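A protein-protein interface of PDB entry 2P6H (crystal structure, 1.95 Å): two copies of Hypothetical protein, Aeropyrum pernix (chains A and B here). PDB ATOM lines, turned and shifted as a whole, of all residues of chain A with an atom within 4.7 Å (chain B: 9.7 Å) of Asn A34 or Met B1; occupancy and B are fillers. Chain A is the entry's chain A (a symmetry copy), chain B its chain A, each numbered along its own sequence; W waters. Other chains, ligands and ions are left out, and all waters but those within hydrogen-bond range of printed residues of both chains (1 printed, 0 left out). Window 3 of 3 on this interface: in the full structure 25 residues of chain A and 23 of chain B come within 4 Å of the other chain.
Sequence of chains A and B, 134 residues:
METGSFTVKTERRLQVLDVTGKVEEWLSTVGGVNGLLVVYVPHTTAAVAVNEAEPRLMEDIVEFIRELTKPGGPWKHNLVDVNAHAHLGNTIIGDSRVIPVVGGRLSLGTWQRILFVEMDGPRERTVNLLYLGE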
ATOM      1  N   GLY A  32     -39.741  26.179 -10.644  1.00  0.00           N
ATOM      2  CA  GLY A  32     -39.022  25.259 -11.517  1.00  0.00           C
ATOM      3  C   GLY A  32     -38.656  23.975 -10.782  1.00  0.00           C
ATOM      4  O   GLY A  32     -38.347  23.982  -9.610  1.00  0.00           O
ATOM      5  N   VAL A  33     -38.731  22.842 -11.508  1.00  0.00           N
ATOM      6  CA  VAL A  33     -38.386  21.597 -10.852  1.00  0.00           C
ATOM      7  C   VAL A  33     -37.045  21.054 -11.366  1.00  0.00           C
ATOM      8  O   VAL A  33     -36.111  20.816 -10.612  1.00  0.00           O
ATOM      9  CB  VAL A  33     -39.526  20.608 -11.123  1.00  0.00           C
ATOM     10  CG1 VAL A  33     -39.167  19.234 -10.559  1.00  0.00           C
ATOM     11  CG2 VAL A  33     -40.804  21.098 -10.469  1.00  0.00           C
ATOM     12  N   ASN A  34     -36.905  20.842 -12.674  1.00  0.00           N
ATOM     13  CA  ASN A  34     -35.642  20.387 -13.255  1.00  0.00           C
ATOM     14  C   ASN A  34     -35.264  21.312 -14.397  1.00  0.00           C
ATOM     15  O   ASN A  34     -36.038  21.534 -15.320  1.00  0.00           O
ATOM     16  CB  ASN A  34     -35.778  18.966 -13.822  1.00  0.00           C
ATOM     17  CG  ASN A  34     -36.254  17.999 -12.764  1.00  0.00           C
ATOM     18  OD1 ASN A  34     -35.553  17.653 -11.817  1.00  0.00           O
ATOM     19  ND2 ASN A  34     -37.489  17.515 -12.984  1.00  0.00           N
ATOM     20  N   GLY A  35     -34.059  21.869 -14.328  1.00  0.00           N
ATOM     21  CA  GLY A  35     -33.613  22.809 -15.364  1.00  0.00           C
ATOM     22  C   GLY A  35     -32.344  23.545 -14.932  1.00  0.00           C
ATOM     23  O   GLY A  35     -31.582  23.061 -14.104  1.00  0.00           O
ATOM     24  N   VAL A 101     -31.009  23.189 -11.323  1.00  0.00           N
ATOM     25  CA  VAL A 101     -32.161  23.108 -10.431  1.00  0.00           C
ATOM     26  C   VAL A 101     -32.599  21.668 -10.645  1.00  0.00           C
ATOM     27  O   VAL A 101     -32.967  21.272 -11.762  1.00  0.00           O
ATOM     28  CB  VAL A 101     -33.288  24.081 -10.842  1.00  0.00           C
ATOM     29  CG1 VAL A 101     -34.529  23.855  -9.965  1.00  0.00           C
ATOM     30  CG2 VAL A 101     -32.803  25.518 -10.683  1.00  0.00           C
ATOM     31  N   VAL A 102     -32.511  20.873  -9.588  1.00  0.00           N
ATOM     32  CA  VAL A 102     -32.860  19.456  -9.691  1.00  0.00           C
ATOM     33  C   VAL A 102     -33.881  19.080  -8.634  1.00  0.00           C
ATOM     34  O   VAL A 102     -33.663  19.234  -7.440  1.00  0.00           O
ATOM     35  CB  VAL A 102     -31.604  18.601  -9.486  1.00  0.00           C
ATOM     36  CG1 VAL A 102     -31.888  17.153  -9.878  1.00  0.00           C
ATOM     37  CG2 VAL A 102     -30.465  19.133 -10.336  1.00  0.00           C
ATOM     38  N   GLY A 103     -35.022  18.562  -9.078  1.00  0.00           N
ATOM     39  CA  GLY A 103     -36.056  18.160  -8.144  1.00  0.00           C
ATOM     40  C   GLY A 103     -36.465  19.323  -7.261  1.00  0.00           C
ATOM     41  O   GLY A 103     -36.681  19.163  -6.059  1.00  0.00           O
ATOM     42  N   TYR A 131     -34.593  31.206 -16.225  1.00  0.00           N
ATOM     43  CA  TYR A 131     -34.836  29.816 -15.871  1.00  0.00           C
ATOM     44  C   TYR A 131     -35.254  29.069 -17.117  1.00  0.00           C
ATOM     45  O   TYR A 131     -36.214  29.450 -17.796  1.00  0.00           O
ATOM     46  CB  TYR A 131     -35.929  29.668 -14.819  1.00  0.00           C
ATOM     47  CG  TYR A 131     -36.181  28.213 -14.505  1.00  0.00           C
ATOM     48  CD1 TYR A 131     -35.235  27.462 -13.807  1.00  0.00           C
ATOM     49  CD2 TYR A 131     -37.318  27.558 -14.983  1.00  0.00           C
ATOM     50  CE1 TYR A 131     -35.409  26.090 -13.598  1.00  0.00           C
ATOM     51  CE2 TYR A 131     -37.498  26.183 -14.777  1.00  0.00           C
ATOM     52  CZ  TYR A 131     -36.540  25.461 -14.091  1.00  0.00           C
ATOM     53  OH  TYR A 131     -36.689  24.102 -13.916  1.00  0.00           O
ATOM     54  N   LEU A 132     -34.533  27.999 -17.409  1.00  0.00           N
ATOM     55  CA  LEU A 132     -34.775  27.198 -18.596  1.00  0.00           C
ATOM     56  C   LEU A 132     -35.011  25.769 -18.161  1.00  0.00           C
ATOM     57  O   LEU A 132     -34.114  25.075 -17.699  1.00  0.00           O
ATOM     58  CB  LEU A 132     -33.547  27.278 -19.525  1.00  0.00           C
ATOM     59  CG  LEU A 132     -33.745  26.592 -20.897  1.00  0.00           C
ATOM     60  CD1 LEU A 132     -34.544  27.457 -21.874  1.00  0.00           C
ATOM     61  CD2 LEU A 132     -32.423  26.270 -21.597  1.00  0.00           C
ATOM     62  N   GLY A 133     -36.237  25.273 -18.304  1.00  0.00           N
ATOM     63  CA  GLY A 133     -36.503  23.902 -17.919  1.00  0.00           C
ATOM     64  C   GLY A 133     -37.950  23.612 -17.579  1.00  0.00           C
ATOM     65  O   GLY A 133     -38.846  24.416 -17.855  1.00  0.00           O
ATOM     66  N   GLU A 134     -38.179  22.442 -16.991  1.00  0.00           N
ATOM     67  CA  GLU A 134     -39.524  22.027 -16.605  1.00  0.00           C
ATOM     68  C   GLU A 134     -39.791  22.295 -15.112  1.00  0.00           C
ATOM     69  O   GLU A 134     -38.873  22.800 -14.417  1.00  0.00           O
ATOM     70  CB  GLU A 134     -39.698  20.534 -16.911  1.00  0.00           C
ATOM     71  CG  GLU A 134     -39.475  19.618 -15.703  1.00  0.00           C
ATOM     72  CD  GLU A 134     -38.806  18.291 -16.056  1.00  0.00           C
ATOM     73  OE1 GLU A 134     -38.295  18.159 -17.189  1.00  0.00           O
ATOM     74  OE2 GLU A 134     -38.775  17.377 -15.198  1.00  0.00           O
ATOM     75  OXT GLU A 134     -40.921  21.985 -14.660  1.00  0.00           O
ATOM     76  N   MET B   1     -33.664  15.920 -18.612  1.00  0.00           N
ATOM     77  CA  MET B   1     -32.211  16.022 -18.307  1.00  0.00           C
ATOM     78  C   MET B   1     -31.742  14.871 -17.433  1.00  0.00           C
ATOM     79  O   MET B   1     -32.531  14.242 -16.725  1.00  0.00           O
ATOM     80  CB  MET B   1     -31.914  17.348 -17.605  1.00  0.00           C
ATOM     81  CG  MET B   1     -32.696  17.545 -16.325  1.00  0.00           C
ATOM     82  SD  MET B   1     -32.454  19.169 -15.594  1.00  0.00           S
ATOM     83  CE  MET B   1     -32.272  18.718 -13.857  1.00  0.00           C
ATOM     84  N   GLU B   2     -30.444  14.602 -17.487  1.00  0.00           N
ATOM     85  CA  GLU B   2     -29.843  13.559 -16.701  1.00  0.00           C
ATOM     86  C   GLU B   2     -28.910  14.164 -15.692  1.00  0.00           C
ATOM     87  O   GLU B   2     -28.381  15.252 -15.838  1.00  0.00           O
ATOM     88  CB  GLU B   2     -29.003  12.636 -17.577  1.00  0.00           C
ATOM     89  CG  GLU B   2     -29.765  12.032 -18.753  1.00  0.00           C
ATOM     90  CD  GLU B   2     -30.833  11.089 -18.244  1.00  0.00           C
ATOM     91  OE1 GLU B   2     -30.684  10.552 -17.158  1.00  0.00           O
ATOM     92  OE2 GLU B   2     -31.791  10.876 -18.958  1.00  0.00           O
ATOM     93  N   THR B   3     -28.690  13.380 -14.659  1.00  0.00           N
ATOM     94  CA  THR B   3     -27.986  13.944 -13.552  1.00  0.00           C
ATOM     95  C   THR B   3     -27.150  12.872 -12.817  1.00  0.00           C
ATOM     96  O   THR B   3     -27.526  11.708 -12.767  1.00  0.00           O
ATOM     97  CB  THR B   3     -29.083  14.540 -12.653  1.00  0.00           C
ATOM     98  OG1 THR B   3     -28.924  15.972 -12.564  1.00  0.00           O
ATOM     99  CG2 THR B   3     -29.115  13.876 -11.284  1.00  0.00           C
ATOM    100  N   GLY B   4     -25.951  13.295 -12.426  1.00  0.00           N
ATOM    101  CA  GLY B   4     -24.973  12.376 -11.877  1.00  0.00           C
ATOM    102  C   GLY B   4     -23.858  13.053 -11.103  1.00  0.00           C
ATOM    103  O   GLY B   4     -23.809  14.278 -10.993  1.00  0.00           O
ATOM    104  N   TRP B  26     -19.626   8.992 -17.436  1.00  0.00           N
ATOM    105  CA  TRP B  26     -21.010   9.323 -17.115  1.00  0.00           C
ATOM    106  C   TRP B  26     -21.751   9.741 -18.375  1.00  0.00           C
ATOM    107  O   TRP B  26     -22.868   9.361 -18.647  1.00  0.00           O
ATOM    108  CB  TRP B  26     -21.031  10.475 -16.094  1.00  0.00           C
ATOM    109  CG  TRP B  26     -22.431  10.784 -15.685  1.00  0.00           C
ATOM    110  CD1 TRP B  26     -23.219  10.057 -14.764  1.00  0.00           C
ATOM    111  CD2 TRP B  26     -23.283  11.855 -16.188  1.00  0.00           C
ATOM    112  NE1 TRP B  26     -24.479  10.539 -14.633  1.00  0.00           N
ATOM    113  CE2 TRP B  26     -24.552  11.702 -15.551  1.00  0.00           C
ATOM    114  CE3 TRP B  26     -23.103  12.886 -17.094  1.00  0.00           C
ATOM    115  CZ2 TRP B  26     -25.578  12.579 -15.842  1.00  0.00           C
ATOM    116  CZ3 TRP B  26     -24.138  13.761 -17.379  1.00  0.00           C
ATOM    117  CH2 TRP B  26     -25.384  13.602 -16.752  1.00  0.00           C
ATOM    118  N   VAL B  30     -25.012   8.038 -20.410  1.00  0.00           N
ATOM    119  CA  VAL B  30     -26.192   8.771 -20.706  1.00  0.00           C
ATOM    120  C   VAL B  30     -26.472   8.772 -22.231  1.00  0.00           C
ATOM    121  O   VAL B  30     -27.612   8.773 -22.678  1.00  0.00           O
ATOM    122  CB  VAL B  30     -25.885  10.147 -20.134  1.00  0.00           C
ATOM    123  CG1 VAL B  30     -26.805  11.187 -20.772  1.00  0.00           C
ATOM    124  CG2 VAL B  30     -26.101  10.141 -18.632  1.00  0.00           C
ATOM    125  N   GLY B  35     -26.631  18.651 -26.950  1.00  0.00           N
ATOM    126  CA  GLY B  35     -27.087  19.295 -25.710  1.00  0.00           C
ATOM    127  C   GLY B  35     -25.927  19.976 -24.983  1.00  0.00           C
ATOM    128  O   GLY B  35     -24.925  20.337 -25.587  1.00  0.00           O
ATOM    129  N   LEU B  36     -26.091  20.192 -23.652  1.00  0.00           N
ATOM    130  CA  LEU B  36     -25.057  20.821 -22.841  1.00  0.00           C
ATOM    131  C   LEU B  36     -24.762  19.969 -21.630  1.00  0.00           C
ATOM    132  O   LEU B  36     -25.629  19.312 -21.068  1.00  0.00           O
ATOM    133  CB  LEU B  36     -25.567  22.125 -22.240  1.00  0.00           C
ATOM    134  CG  LEU B  36     -25.930  23.243 -23.196  1.00  0.00           C
ATOM    135  CD1 LEU B  36     -26.575  24.349 -22.348  1.00  0.00           C
ATOM    136  CD2 LEU B  36     -24.736  23.891 -23.894  1.00  0.00           C
ATOM    137  N   LEU B  37     -23.492  19.954 -21.261  1.00  0.00           N
ATOM    138  CA  LEU B  37     -23.133  19.283 -20.071  1.00  0.00           C
ATOM    139  C   LEU B  37     -22.679  20.346 -19.109  1.00  0.00           C
ATOM    140  O   LEU B  37     -21.984  21.284 -19.478  1.00  0.00           O
ATOM    141  CB  LEU B  37     -21.970  18.372 -20.419  1.00  0.00           C
ATOM    142  CG  LEU B  37     -21.227  17.944 -19.167  1.00  0.00           C
ATOM    143  CD1 LEU B  37     -22.033  16.901 -18.401  1.00  0.00           C
ATOM    144  CD2 LEU B  37     -19.841  17.356 -19.434  1.00  0.00           C
ATOM    145  N   VAL B  38     -23.138  20.253 -17.862  1.00  0.00           N
ATOM    146  CA  VAL B  38     -22.639  21.196 -16.860  1.00  0.00           C
ATOM    147  C   VAL B  38     -21.866  20.425 -15.839  1.00  0.00           C
ATOM    148  O   VAL B  38     -22.352  19.475 -15.241  1.00  0.00           O
ATOM    149  CB  VAL B  38     -23.785  21.932 -16.128  1.00  0.00           C
ATOM    150  CG1 VAL B  38     -23.206  22.925 -15.121  1.00  0.00           C
ATOM    151  CG2 VAL B  38     -24.644  22.681 -17.130  1.00  0.00           C
ATOM    152  N   TYR B  40     -19.905  20.868 -12.413  1.00  0.00           N
ATOM    153  CA  TYR B  40     -19.803  21.817 -11.321  1.00  0.00           C
ATOM    154  C   TYR B  40     -19.498  21.129 -10.001  1.00  0.00           C
ATOM    155  O   TYR B  40     -19.789  19.953  -9.791  1.00  0.00           O
ATOM    156  CB  TYR B  40     -21.098  22.655 -11.228  1.00  0.00           C
ATOM    157  CG  TYR B  40     -22.308  21.819 -10.936  1.00  0.00           C
ATOM    158  CD1 TYR B  40     -22.801  20.918 -11.881  1.00  0.00           C
ATOM    159  CD2 TYR B  40     -23.008  21.994  -9.737  1.00  0.00           C
ATOM    160  CE1 TYR B  40     -23.960  20.189 -11.627  1.00  0.00           C
ATOM    161  CE2 TYR B  40     -24.172  21.270  -9.486  1.00  0.00           C
ATOM    162  CZ  TYR B  40     -24.638  20.358 -10.433  1.00  0.00           C
ATOM    163  OH  TYR B  40     -25.797  19.641 -10.186  1.00  0.00           O
ATOM    164  N   LEU B 129     -22.705  16.499 -12.103  1.00  0.00           N
ATOM    165  CA  LEU B 129     -22.857  16.562 -13.553  1.00  0.00           C
ATOM    166  C   LEU B 129     -24.324  16.647 -13.938  1.00  0.00           C
ATOM    167  O   LEU B 129     -25.185  16.022 -13.319  1.00  0.00           O
ATOM    168  CB  LEU B 129     -22.246  15.314 -14.212  1.00  0.00           C
ATOM    169  CG  LEU B 129     -20.806  14.953 -13.817  1.00  0.00           C
ATOM    170  CD1 LEU B 129     -20.456  13.546 -14.253  1.00  0.00           C
ATOM    171  CD2 LEU B 129     -19.846  15.963 -14.426  1.00  0.00           C
ATOM    172  N   LEU B 130     -24.599  17.437 -14.968  1.00  0.00           N
ATOM    173  CA  LEU B 130     -25.961  17.629 -15.465  1.00  0.00           C
ATOM    174  C   LEU B 130     -25.943  17.630 -16.980  1.00  0.00           C
ATOM    175  O   LEU B 130     -25.180  18.345 -17.617  1.00  0.00           O
ATOM    176  CB  LEU B 130     -26.528  18.968 -14.944  1.00  0.00           C
ATOM    177  CG  LEU B 130     -27.969  19.279 -15.431  1.00  0.00           C
ATOM    178  CD1 LEU B 130     -28.712  20.228 -14.491  1.00  0.00           C
ATOM    179  CD2 LEU B 130     -27.997  19.934 -16.812  1.00  0.00           C
ATOM    180  N   TYR B 131     -26.803  16.822 -17.586  1.00  0.00           N
ATOM    181  CA  TYR B 131     -26.888  16.789 -19.037  1.00  0.00           C
ATOM    182  C   TYR B 131     -28.278  17.218 -19.448  1.00  0.00           C
ATOM    183  O   TYR B 131     -29.278  16.643 -19.007  1.00  0.00           O
ATOM    184  CB  TYR B 131     -26.616  15.398 -19.602  1.00  0.00           C
ATOM    185  CG  TYR B 131     -26.751  15.393 -21.107  1.00  0.00           C
ATOM    186  CD1 TYR B 131     -25.809  16.039 -21.908  1.00  0.00           C
ATOM    187  CD2 TYR B 131     -27.865  14.826 -21.730  1.00  0.00           C
ATOM    188  CE1 TYR B 131     -25.974  16.128 -23.293  1.00  0.00           C
ATOM    189  CE2 TYR B 131     -28.038  14.913 -23.118  1.00  0.00           C
ATOM    190  CZ  TYR B 131     -27.092  15.567 -23.887  1.00  0.00           C
ATOM    191  OH  TYR B 131     -27.271  15.691 -25.247  1.00  0.00           O
ATOM    192  N   LEU B 132     -28.333  18.229 -20.300  1.00  0.00           N
ATOM    193  CA  LEU B 132     -29.592  18.792 -20.758  1.00  0.00           C
ATOM    194  C   LEU B 132     -29.613  18.735 -22.270  1.00  0.00           C
ATOM    195  O   LEU B 132     -28.881  19.438 -22.955  1.00  0.00           O
ATOM    196  CB  LEU B 132     -29.702  20.253 -20.277  1.00  0.00           C
ATOM    197  CG  LEU B 132     -31.070  20.915 -20.568  1.00  0.00           C
ATOM    198  CD1 LEU B 132     -32.146  20.498 -19.562  1.00  0.00           C
ATOM    199  CD2 LEU B 132     -31.013  22.442 -20.523  1.00  0.00           C
ATOM    200  N   GLY B 133     -30.467  17.893 -22.844  1.00  0.00           N
ATOM    201  CA  GLY B 133     -30.535  17.821 -24.290  1.00  0.00           C
ATOM    202  C   GLY B 133     -31.067  16.510 -24.831  1.00  0.00           C
ATOM    203  O   GLY B 133     -31.623  15.691 -24.093  1.00  0.00           O
ATOM    204  N   GLU B 134     -30.909  16.322 -26.138  1.00  0.00           N
ATOM    205  CA  GLU B 134     -31.373  15.106 -26.800  1.00  0.00           C
ATOM    206  C   GLU B 134     -30.225  14.098 -26.995  1.00  0.00           C
ATOM    207  O   GLU B 134     -29.072  14.413 -26.602  1.00  0.00           O
ATOM    208  CB  GLU B 134     -31.987  15.473 -28.156  1.00  0.00           C
ATOM    209  CG  GLU B 134     -31.032  15.304 -29.342  1.00  0.00           C
ATOM    210  CD  GLU B 134     -31.213  16.364 -30.428  1.00  0.00           C
ATOM    211  OE1 GLU B 134     -31.909  17.372 -30.175  1.00  0.00           O
ATOM    212  OE2 GLU B 134     -30.649  16.202 -31.536  1.00  0.00           O
ATOM    213  OXT GLU B 134     -30.501  13.006 -27.550  1.00  0.00           O
HETATM  214  O   HOH W   1     -36.429  16.258 -16.976  1.00  0.00           O
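The side-chain sulfur of Met B1 is in hydrogen-bond range of the backbone NH of Gly A35 (3.4 Å).
The backbone NH (N) of Gly A103 sits at hydrogen-bond distance from the side-chain amide oxygen (OD1) of Asn A34, at 2.9 Å.
OH of Tyr A131 sits at hydrogen-bond distance from O of Asn A34, 3.0 Å away.
ND2 of Asn A34 sits at hydrogen-bond distance from OE2 of Glu A134 (2.6 Å).
The backbone NH (N) of Val A101 sits at hydrogen-bond distance from the backbone carbonyl oxygen (O) of Gly A35, 2.8 Å away.
The side-chain hydroxyl of Tyr A131 lies within hydrogen-bond range of the backbone NH of Gly A35 (3.5 Å).
Among the printed residues, pairs that only touch across the chains: Val A101 with Met B1, Asn A34 with Met B1 and Val A102 with Met B1.
Of chain B, only Met B1 (3.5 Å) comes within 4 Å of Asn A34.
Of chain A, only Asn A34, Gly A35, Val A101 and Val A102 come within 4 Å of Met B1.
No residue of chain B comes within 4 Å of Val A33.
Gly A35 touches one residue of chain B.
No residue of chain B comes within 4 Å of Gly A133.
No residue of chain B comes within 4 Å of Glu A134.
Of the printed residues of chain B, Val A101 touches Met B1 (3.4 Å).
The nearest printed residue of chain B that does not touch Val A101 is Leu B130 (4.9 Å).
Of the 11 printed residues of chain A, 4 touch a printed residue of chain B.
Printed residues of chain A that touch a printed residue of chain B: Asn A34, Gly A35, Val A101 and Val A102.
Hydrophobic or aromatic side chains of chain A that line the printed part of chain B: Val A102.
Of the 17 printed residues of chain B, 1 touches a printed residue of chain A.
Printed residues of chain B that touch a printed residue of chain A: Met B1.
Hydrophobic or aromatic side chains of chain B that line the printed part of chain A: Met B1.
Positions printed for both chains: 35, 131, 132, 133 and 134.
Of the 4 pairs that touch across the chains among the printed residues, none has its exchanged pair printed and touching as well.
Water W1 lies within hydrogen-bond range of the side-chain carboxylate of Glu A134 (2.7 Å) and the backbone NH of Met B1 (3.2 Å).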
